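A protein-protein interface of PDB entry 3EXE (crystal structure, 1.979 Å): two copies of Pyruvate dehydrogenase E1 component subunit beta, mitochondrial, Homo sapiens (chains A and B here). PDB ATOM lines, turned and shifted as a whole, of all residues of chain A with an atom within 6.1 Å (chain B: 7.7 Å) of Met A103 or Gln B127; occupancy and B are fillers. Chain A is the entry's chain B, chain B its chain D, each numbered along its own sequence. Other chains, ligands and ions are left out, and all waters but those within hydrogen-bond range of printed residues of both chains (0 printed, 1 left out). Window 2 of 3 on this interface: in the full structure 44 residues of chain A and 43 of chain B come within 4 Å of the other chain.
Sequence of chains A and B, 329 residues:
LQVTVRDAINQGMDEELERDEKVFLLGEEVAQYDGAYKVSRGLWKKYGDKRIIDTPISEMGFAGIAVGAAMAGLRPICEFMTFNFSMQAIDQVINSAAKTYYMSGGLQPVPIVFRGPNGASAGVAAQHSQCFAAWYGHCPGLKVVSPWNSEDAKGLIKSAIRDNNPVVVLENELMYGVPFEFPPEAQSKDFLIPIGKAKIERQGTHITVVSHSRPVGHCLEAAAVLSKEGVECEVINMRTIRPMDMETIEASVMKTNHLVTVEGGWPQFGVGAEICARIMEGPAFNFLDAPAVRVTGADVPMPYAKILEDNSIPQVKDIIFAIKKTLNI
Of chain B, only Ala B126 and Gln B127 come within 4 Å of Met A103.
Gln B127 touches just these residues of chain A: Asn A95 (2.8 Å) and Met A103 (3.8 Å).
Of the printed residues of chain A, Ala B126 touches Lys A99 (3.0 Å) and Met A103 (3.7 Å).
Printed residues of chain A within 4 Å of Met B87: Asn A95.
Of the printed residues of chain A, Pro B301 touches Tyr A102 (3.1 Å).
Val B124 touches none of the printed residues of chain A.
Asn B84 touches none of the printed residues of chain A.
The nearest residue of chain A that does not touch Gln B127 is Lys A99 (4.1 Å).
Asn A95 touches Met B87 (ND2 to CE, 3.2 Å).
Tyr A102 touches Pro B301.
Tyr A102 touches Pro B303.
Met A103 touches Ala B126 (CG to CB, 3.7 Å).
CE of Met A103 touches NE2 of Gln B127, 3.8 Å away.
The side-chain amide oxygen of Asn B84 lies close to the backbone carbonyl oxygen of Gln B127 (3.3 Å).
NZ of Lys A99 lies within hydrogen-bond range of OD1 of Asn A95 (2.6 Å).
The backbone NH (N) of Ala B126 sits at hydrogen-bond distance from the backbone carbonyl oxygen (O) of Met B302 (3.2 Å).
The backbone NH (N) of Gln B130 is in hydrogen-bond range of the side-chain amide oxygen (OD1) of Asn B84 (3.0 Å).
Of the 10 printed residues of chain A, 4 touch a printed residue of chain B.
Among the printed residues, no Asp or Glu carboxylate lies within 4 Å of a Lys or Arg side-chain nitrogen of the other chain.
No position is printed for both chains.
Of the 8 pairs that touch across the chains among the printed residues, none has its exchanged pair printed and touching as well.
The side-chain amide oxygen (OE1) of Gln B130 sits at hydrogen-bond distance from the side-chain amino group (NZ) of Lys A99.
The backbone carbonyl oxygen of Ala B126 sits at hydrogen-bond distance from the side-chain amino group of Lys A99 (3.0 Å).
O of Asn A95 lies within hydrogen-bond range of NE2 of Gln B127 (2.8 Å).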
ATOM      1  N   ASN A  95      17.125 -16.349  27.884  1.00  0.00           N
ATOM      2  CA  ASN A  95      16.190 -16.870  28.860  1.00  0.00           C
ATOM      3  C   ASN A  95      15.308 -15.818  29.536  1.00  0.00           C
ATOM      4  O   ASN A  95      14.121 -16.093  29.814  1.00  0.00           O
ATOM      5  CB  ASN A  95      16.897 -17.799  29.880  1.00  0.00           C
ATOM      6  CG  ASN A  95      17.042 -19.193  29.370  1.00  0.00           C
ATOM      7  OD1 ASN A  95      16.275 -19.631  28.507  1.00  0.00           O
ATOM      8  ND2 ASN A  95      18.010 -19.904  29.885  1.00  0.00           N
ATOM      9  N   SER A  96      15.822 -14.598  29.754  1.00  0.00           N
ATOM     10  CA  SER A  96      14.980 -13.563  30.363  1.00  0.00           C
ATOM     11  C   SER A  96      14.241 -12.710  29.379  1.00  0.00           C
ATOM     12  O   SER A  96      13.129 -12.246  29.703  1.00  0.00           O
ATOM     13  CB  SER A  96      15.764 -12.618  31.300  1.00  0.00           C
ATOM     14  OG  SER A  96      16.407 -13.353  32.341  1.00  0.00           O
ATOM     15  N   LYS A  99      12.384 -15.444  25.530  1.00  0.00           N
ATOM     16  CA  LYS A  99      11.359 -16.470  25.736  1.00  0.00           C
ATOM     17  C   LYS A  99      10.147 -15.940  26.540  1.00  0.00           C
ATOM     18  O   LYS A  99       9.147 -16.642  26.720  1.00  0.00           O
ATOM     19  CB  LYS A  99      12.019 -17.636  26.496  1.00  0.00           C
ATOM     20  CG  LYS A  99      13.078 -18.351  25.650  1.00  0.00           C
ATOM     21  CD  LYS A  99      13.672 -19.487  26.401  1.00  0.00           C
ATOM     22  CE  LYS A  99      14.735 -20.235  25.516  1.00  0.00           C
ATOM     23  NZ  LYS A  99      15.636 -21.059  26.379  1.00  0.00           N
ATOM     24  N   THR A 100      10.261 -14.747  27.099  1.00  0.00           N
ATOM     25  CA  THR A 100       9.306 -14.369  28.152  1.00  0.00           C
ATOM     26  C   THR A 100       7.832 -14.117  27.731  1.00  0.00           C
ATOM     27  O   THR A 100       6.875 -14.530  28.436  1.00  0.00           O
ATOM     28  CB  THR A 100       9.853 -13.199  29.004  1.00  0.00           C
ATOM     29  OG1 THR A 100      10.975 -13.674  29.776  1.00  0.00           O
ATOM     30  CG2 THR A 100       8.735 -12.614  29.949  1.00  0.00           C
ATOM     31  N   TYR A 101       7.651 -13.380  26.632  1.00  0.00           N
ATOM     32  CA  TYR A 101       6.330 -13.169  26.087  1.00  0.00           C
ATOM     33  C   TYR A 101       5.608 -14.505  25.889  1.00  0.00           C
ATOM     34  O   TYR A 101       4.459 -14.635  26.265  1.00  0.00           O
ATOM     35  CB  TYR A 101       6.377 -12.349  24.770  1.00  0.00           C
ATOM     36  CG  TYR A 101       5.027 -11.748  24.343  1.00  0.00           C
ATOM     37  CD1 TYR A 101       4.390 -10.768  25.098  1.00  0.00           C
ATOM     38  CD2 TYR A 101       4.405 -12.201  23.207  1.00  0.00           C
ATOM     39  CE1 TYR A 101       3.157 -10.217  24.705  1.00  0.00           C
ATOM     40  CE2 TYR A 101       3.172 -11.699  22.805  1.00  0.00           C
ATOM     41  CZ  TYR A 101       2.558 -10.723  23.545  1.00  0.00           C
ATOM     42  OH  TYR A 101       1.340 -10.261  23.061  1.00  0.00           O
ATOM     43  N   TYR A 102       6.300 -15.480  25.323  1.00  0.00           N
ATOM     44  CA  TYR A 102       5.723 -16.828  25.057  1.00  0.00           C
ATOM     45  C   TYR A 102       5.434 -17.583  26.358  1.00  0.00           C
ATOM     46  O   TYR A 102       4.321 -18.109  26.586  1.00  0.00           O
ATOM     47  CB  TYR A 102       6.711 -17.670  24.247  1.00  0.00           C
ATOM     48  CG  TYR A 102       6.139 -19.006  23.830  1.00  0.00           C
ATOM     49  CD1 TYR A 102       5.347 -19.107  22.651  1.00  0.00           C
ATOM     50  CD2 TYR A 102       6.319 -20.144  24.625  1.00  0.00           C
ATOM     51  CE1 TYR A 102       4.811 -20.356  22.242  1.00  0.00           C
ATOM     52  CE2 TYR A 102       5.780 -21.376  24.260  1.00  0.00           C
ATOM     53  CZ  TYR A 102       5.043 -21.478  23.040  1.00  0.00           C
ATOM     54  OH  TYR A 102       4.493 -22.676  22.619  1.00  0.00           O
ATOM     55  N   MET A 103       6.431 -17.641  27.222  1.00  0.00           N
ATOM     56  CA  MET A 103       6.192 -18.283  28.534  1.00  0.00           C
ATOM     57  C   MET A 103       5.020 -17.714  29.350  1.00  0.00           C
ATOM     58  O   MET A 103       4.349 -18.458  30.072  1.00  0.00           O
ATOM     59  CB  MET A 103       7.437 -18.280  29.386  1.00  0.00           C
ATOM     60  CG  MET A 103       8.552 -19.181  28.812  1.00  0.00           C
ATOM     61  SD  MET A 103       9.927 -19.357  29.988  1.00  0.00           S
ATOM     62  CE  MET A 103      10.509 -17.652  30.092  1.00  0.00           C
ATOM     63  N   SER A 104       4.865 -16.396  29.308  1.00  0.00           N
ATOM     64  CA  SER A 104       3.861 -15.673  30.057  1.00  0.00           C
ATOM     65  C   SER A 104       2.507 -15.709  29.370  1.00  0.00           C
ATOM     66  O   SER A 104       1.547 -15.105  29.869  1.00  0.00           O
ATOM     67  CB  SER A 104       4.269 -14.197  30.285  1.00  0.00           C
ATOM     68  OG  SER A 104       4.184 -13.435  29.074  1.00  0.00           O
ATOM     69  N   GLY A 105       2.425 -16.425  28.232  1.00  0.00           N
ATOM     70  CA  GLY A 105       1.235 -16.437  27.377  1.00  0.00           C
ATOM     71  C   GLY A 105       0.808 -15.047  26.921  1.00  0.00           C
ATOM     72  O   GLY A 105      -0.389 -14.756  26.931  1.00  0.00           O
ATOM     73  N   GLY A 106       1.763 -14.202  26.502  1.00  0.00           N
ATOM     74  CA  GLY A 106       1.395 -12.885  25.967  1.00  0.00           C
ATOM     75  C   GLY A 106       1.102 -11.799  27.010  1.00  0.00           C
ATOM     76  O   GLY A 106       0.578 -10.779  26.672  1.00  0.00           O
ATOM     77  N   THR B  82      22.140 -28.745  33.698  1.00  0.00           N
ATOM     78  CA  THR B  82      21.722 -28.932  32.292  1.00  0.00           C
ATOM     79  C   THR B  82      22.546 -27.930  31.475  1.00  0.00           C
ATOM     80  O   THR B  82      23.049 -26.911  32.004  1.00  0.00           O
ATOM     81  CB  THR B  82      20.173 -28.622  32.046  1.00  0.00           C
ATOM     82  OG1 THR B  82      19.914 -27.230  32.310  1.00  0.00           O
ATOM     83  CG2 THR B  82      19.307 -29.410  33.005  1.00  0.00           C
ATOM     84  N   PHE B  83      22.620 -28.141  30.168  1.00  0.00           N
ATOM     85  CA  PHE B  83      23.333 -27.173  29.324  1.00  0.00           C
ATOM     86  C   PHE B  83      22.623 -25.812  29.227  1.00  0.00           C
ATOM     87  O   PHE B  83      23.262 -24.794  28.933  1.00  0.00           O
ATOM     88  CB  PHE B  83      23.727 -27.805  27.946  1.00  0.00           C
ATOM     89  CG  PHE B  83      25.058 -28.437  27.978  1.00  0.00           C
ATOM     90  CD1 PHE B  83      25.214 -29.793  28.273  1.00  0.00           C
ATOM     91  CD2 PHE B  83      26.209 -27.651  27.789  1.00  0.00           C
ATOM     92  CE1 PHE B  83      26.513 -30.379  28.352  1.00  0.00           C
ATOM     93  CE2 PHE B  83      27.493 -28.228  27.898  1.00  0.00           C
ATOM     94  CZ  PHE B  83      27.647 -29.599  28.160  1.00  0.00           C
ATOM     95  N   ASN B  84      21.314 -25.736  29.546  1.00  0.00           N
ATOM     96  CA  ASN B  84      20.724 -24.406  29.693  1.00  0.00           C
ATOM     97  C   ASN B  84      21.569 -23.472  30.569  1.00  0.00           C
ATOM     98  O   ASN B  84      21.675 -22.251  30.310  1.00  0.00           O
ATOM     99  CB  ASN B  84      19.261 -24.473  30.250  1.00  0.00           C
ATOM    100  CG  ASN B  84      18.425 -25.492  29.501  1.00  0.00           C
ATOM    101  OD1 ASN B  84      17.969 -25.188  28.422  1.00  0.00           O
ATOM    102  ND2 ASN B  84      18.270 -26.714  30.052  1.00  0.00           N
ATOM    103  N   PHE B  85      22.049 -24.018  31.678  1.00  0.00           N
ATOM    104  CA  PHE B  85      22.782 -23.220  32.691  1.00  0.00           C
ATOM    105  C   PHE B  85      24.215 -22.967  32.236  1.00  0.00           C
ATOM    106  O   PHE B  85      24.893 -22.134  32.817  1.00  0.00           O
ATOM    107  CB  PHE B  85      22.798 -23.921  34.062  1.00  0.00           C
ATOM    108  CG  PHE B  85      21.486 -24.522  34.457  1.00  0.00           C
ATOM    109  CD1 PHE B  85      20.320 -23.872  34.164  1.00  0.00           C
ATOM    110  CD2 PHE B  85      21.450 -25.770  35.134  1.00  0.00           C
ATOM    111  CE1 PHE B  85      19.101 -24.423  34.525  1.00  0.00           C
ATOM    112  CE2 PHE B  85      20.225 -26.325  35.490  1.00  0.00           C
ATOM    113  CZ  PHE B  85      19.062 -25.662  35.171  1.00  0.00           C
ATOM    114  N   MET B  87      24.819 -21.391  29.608  1.00  0.00           N
ATOM    115  CA  MET B  87      24.849 -20.037  28.985  1.00  0.00           C
ATOM    116  C   MET B  87      25.585 -19.038  29.890  1.00  0.00           C
ATOM    117  O   MET B  87      26.303 -18.177  29.394  1.00  0.00           O
ATOM    118  CB  MET B  87      23.460 -19.539  28.557  1.00  0.00           C
ATOM    119  CG  MET B  87      22.947 -20.302  27.278  1.00  0.00           C
ATOM    120  SD  MET B  87      21.649 -19.344  26.497  1.00  0.00           S
ATOM    121  CE  MET B  87      20.340 -19.779  27.632  1.00  0.00           C
ATOM    122  N   VAL B 124       9.393 -29.512  31.376  1.00  0.00           N
ATOM    123  CA  VAL B 124      10.325 -28.582  32.084  1.00  0.00           C
ATOM    124  C   VAL B 124      10.314 -27.167  31.528  1.00  0.00           C
ATOM    125  O   VAL B 124      10.957 -26.294  32.083  1.00  0.00           O
ATOM    126  CB  VAL B 124      11.819 -29.114  32.173  1.00  0.00           C
ATOM    127  CG1 VAL B 124      11.788 -30.462  32.943  1.00  0.00           C
ATOM    128  CG2 VAL B 124      12.468 -29.264  30.767  1.00  0.00           C
ATOM    129  N   ALA B 125       9.598 -26.986  30.435  1.00  0.00           N
ATOM    130  CA  ALA B 125       9.322 -25.683  29.838  1.00  0.00           C
ATOM    131  C   ALA B 125      10.543 -24.975  29.274  1.00  0.00           C
ATOM    132  O   ALA B 125      11.577 -25.571  29.057  1.00  0.00           O
ATOM    133  CB  ALA B 125       8.477 -24.741  30.762  1.00  0.00           C
ATOM    134  N   ALA B 126      10.356 -23.728  28.917  1.00  0.00           N
ATOM    135  CA  ALA B 126      11.189 -23.128  27.875  1.00  0.00           C
ATOM    136  C   ALA B 126      12.632 -22.815  28.298  1.00  0.00           C
ATOM    137  O   ALA B 126      13.519 -22.945  27.474  1.00  0.00           O
ATOM    138  CB  ALA B 126      10.505 -21.895  27.289  1.00  0.00           C
ATOM    139  N   GLN B 127      12.871 -22.457  29.570  1.00  0.00           N
ATOM    140  CA  GLN B 127      14.233 -22.163  30.047  1.00  0.00           C
ATOM    141  C   GLN B 127      15.045 -23.409  30.304  1.00  0.00           C
ATOM    142  O   GLN B 127      16.254 -23.341  30.517  1.00  0.00           O
ATOM    143  CB  GLN B 127      14.208 -21.274  31.309  1.00  0.00           C
ATOM    144  CG  GLN B 127      13.723 -19.843  30.997  1.00  0.00           C
ATOM    145  CD  GLN B 127      13.623 -18.985  32.255  1.00  0.00           C
ATOM    146  OE1 GLN B 127      13.420 -19.514  33.344  1.00  0.00           O
ATOM    147  NE2 GLN B 127      13.685 -17.659  32.095  1.00  0.00           N
ATOM    148  N   HIS B 128      14.375 -24.558  30.292  1.00  0.00           N
ATOM    149  CA  HIS B 128      15.041 -25.788  30.613  1.00  0.00           C
ATOM    150  C   HIS B 128      15.051 -26.855  29.531  1.00  0.00           C
ATOM    151  O   HIS B 128      15.425 -27.995  29.816  1.00  0.00           O
ATOM    152  CB  HIS B 128      14.435 -26.409  31.873  1.00  0.00           C
ATOM    153  CG  HIS B 128      14.692 -25.595  33.081  1.00  0.00           C
ATOM    154  ND1 HIS B 128      14.186 -24.322  33.243  1.00  0.00           N
ATOM    155  CD2 HIS B 128      15.422 -25.865  34.195  1.00  0.00           C
ATOM    156  CE1 HIS B 128      14.609 -23.830  34.402  1.00  0.00           C
ATOM    157  NE2 HIS B 128      15.342 -24.755  34.999  1.00  0.00           N
ATOM    158  N   SER B 129      14.674 -26.490  28.316  1.00  0.00           N
ATOM    159  CA  SER B 129      14.540 -27.492  27.248  1.00  0.00           C
ATOM    160  C   SER B 129      15.445 -27.259  26.080  1.00  0.00           C
ATOM    161  O   SER B 129      15.268 -27.933  25.066  1.00  0.00           O
ATOM    162  CB  SER B 129      13.117 -27.471  26.651  1.00  0.00           C
ATOM    163  OG  SER B 129      12.176 -27.778  27.639  1.00  0.00           O
ATOM    164  N   GLN B 130      16.344 -26.262  26.152  1.00  0.00           N
ATOM    165  CA  GLN B 130      17.044 -25.812  24.894  1.00  0.00           C
ATOM    166  C   GLN B 130      18.198 -26.797  24.498  1.00  0.00           C
ATOM    167  O   GLN B 130      18.937 -27.270  25.350  1.00  0.00           O
ATOM    168  CB  GLN B 130      17.572 -24.369  25.069  1.00  0.00           C
ATOM    169  CG  GLN B 130      18.322 -23.734  23.849  1.00  0.00           C
ATOM    170  CD  GLN B 130      18.685 -22.297  24.185  1.00  0.00           C
ATOM    171  OE1 GLN B 130      18.106 -21.735  25.107  1.00  0.00           O
ATOM    172  NE2 GLN B 130      19.613 -21.682  23.417  1.00  0.00           N
ATOM    173  N   PHE B 132      21.801 -27.225  22.676  1.00  0.00           N
ATOM    174  CA  PHE B 132      22.953 -26.391  22.362  1.00  0.00           C
ATOM    175  C   PHE B 132      23.917 -27.036  21.334  1.00  0.00           C
ATOM    176  O   PHE B 132      25.009 -26.545  21.120  1.00  0.00           O
ATOM    177  CB  PHE B 132      23.674 -26.009  23.679  1.00  0.00           C
ATOM    178  CG  PHE B 132      22.837 -25.116  24.543  1.00  0.00           C
ATOM    179  CD1 PHE B 132      21.890 -25.667  25.431  1.00  0.00           C
ATOM    180  CD2 PHE B 132      22.950 -23.748  24.442  1.00  0.00           C
ATOM    181  CE1 PHE B 132      21.065 -24.837  26.241  1.00  0.00           C
ATOM    182  CE2 PHE B 132      22.137 -22.892  25.269  1.00  0.00           C
ATOM    183  CZ  PHE B 132      21.179 -23.465  26.146  1.00  0.00           C
ATOM    184  N   PRO B 301       9.708 -21.314  21.711  1.00  0.00           N
ATOM    185  CA  PRO B 301      10.252 -21.701  23.031  1.00  0.00           C
ATOM    186  C   PRO B 301       9.396 -22.900  23.517  1.00  0.00           C
ATOM    187  O   PRO B 301       8.238 -22.902  23.244  1.00  0.00           O
ATOM    188  CB  PRO B 301       9.880 -20.515  23.891  1.00  0.00           C
ATOM    189  CG  PRO B 301       9.812 -19.307  22.873  1.00  0.00           C
ATOM    190  CD  PRO B 301       9.128 -19.959  21.715  1.00  0.00           C
ATOM    191  N   MET B 302       9.943 -23.819  24.301  1.00  0.00           N
ATOM    192  CA  MET B 302       9.235 -25.067  24.613  1.00  0.00           C
ATOM    193  C   MET B 302       8.062 -24.791  25.536  1.00  0.00           C
ATOM    194  O   MET B 302       8.239 -24.278  26.640  1.00  0.00           O
ATOM    195  CB  MET B 302      10.206 -26.072  25.269  1.00  0.00           C
ATOM    196  CG  MET B 302       9.603 -27.496  25.599  1.00  0.00           C
ATOM    197  SD  MET B 302       9.233 -28.289  23.985  1.00  0.00           S
ATOM    198  CE  MET B 302      10.896 -28.743  23.346  1.00  0.00           C
ATOM    199  N   PRO B 303       6.845 -25.162  25.107  1.00  0.00           N
ATOM    200  CA  PRO B 303       5.697 -24.996  25.972  1.00  0.00           C
ATOM    201  C   PRO B 303       5.616 -26.136  27.027  1.00  0.00           C
ATOM    202  O   PRO B 303       6.045 -27.273  26.791  1.00  0.00           O
ATOM    203  CB  PRO B 303       4.487 -25.101  25.012  1.00  0.00           C
ATOM    204  CG  PRO B 303       5.016 -25.999  23.863  1.00  0.00           C
ATOM    205  CD  PRO B 303       6.514 -25.717  23.778  1.00  0.00           C
ATOM    206  N   TYR B 304       4.976 -25.813  28.139  1.00  0.00           N
ATOM    207  CA  TYR B 304       4.720 -26.735  29.234  1.00  0.00           C
ATOM    208  C   TYR B 304       3.637 -27.817  28.955  1.00  0.00           C
ATOM    209  O   TYR B 304       3.868 -28.991  29.225  1.00  0.00           O
ATOM    210  CB  TYR B 304       4.265 -25.908  30.429  1.00  0.00           C
ATOM    211  CG  TYR B 304       3.861 -26.768  31.597  1.00  0.00           C
ATOM    212  CD1 TYR B 304       4.757 -27.696  32.138  1.00  0.00           C
ATOM    213  CD2 TYR B 304       2.564 -26.695  32.131  1.00  0.00           C
ATOM    214  CE1 TYR B 304       4.437 -28.490  33.201  1.00  0.00           C
ATOM    215  CE2 TYR B 304       2.217 -27.520  33.239  1.00  0.00           C
ATOM    216  CZ  TYR B 304       3.167 -28.376  33.777  1.00  0.00           C
ATOM    217  OH  TYR B 304       2.843 -29.173  34.868  1.00  0.00           O
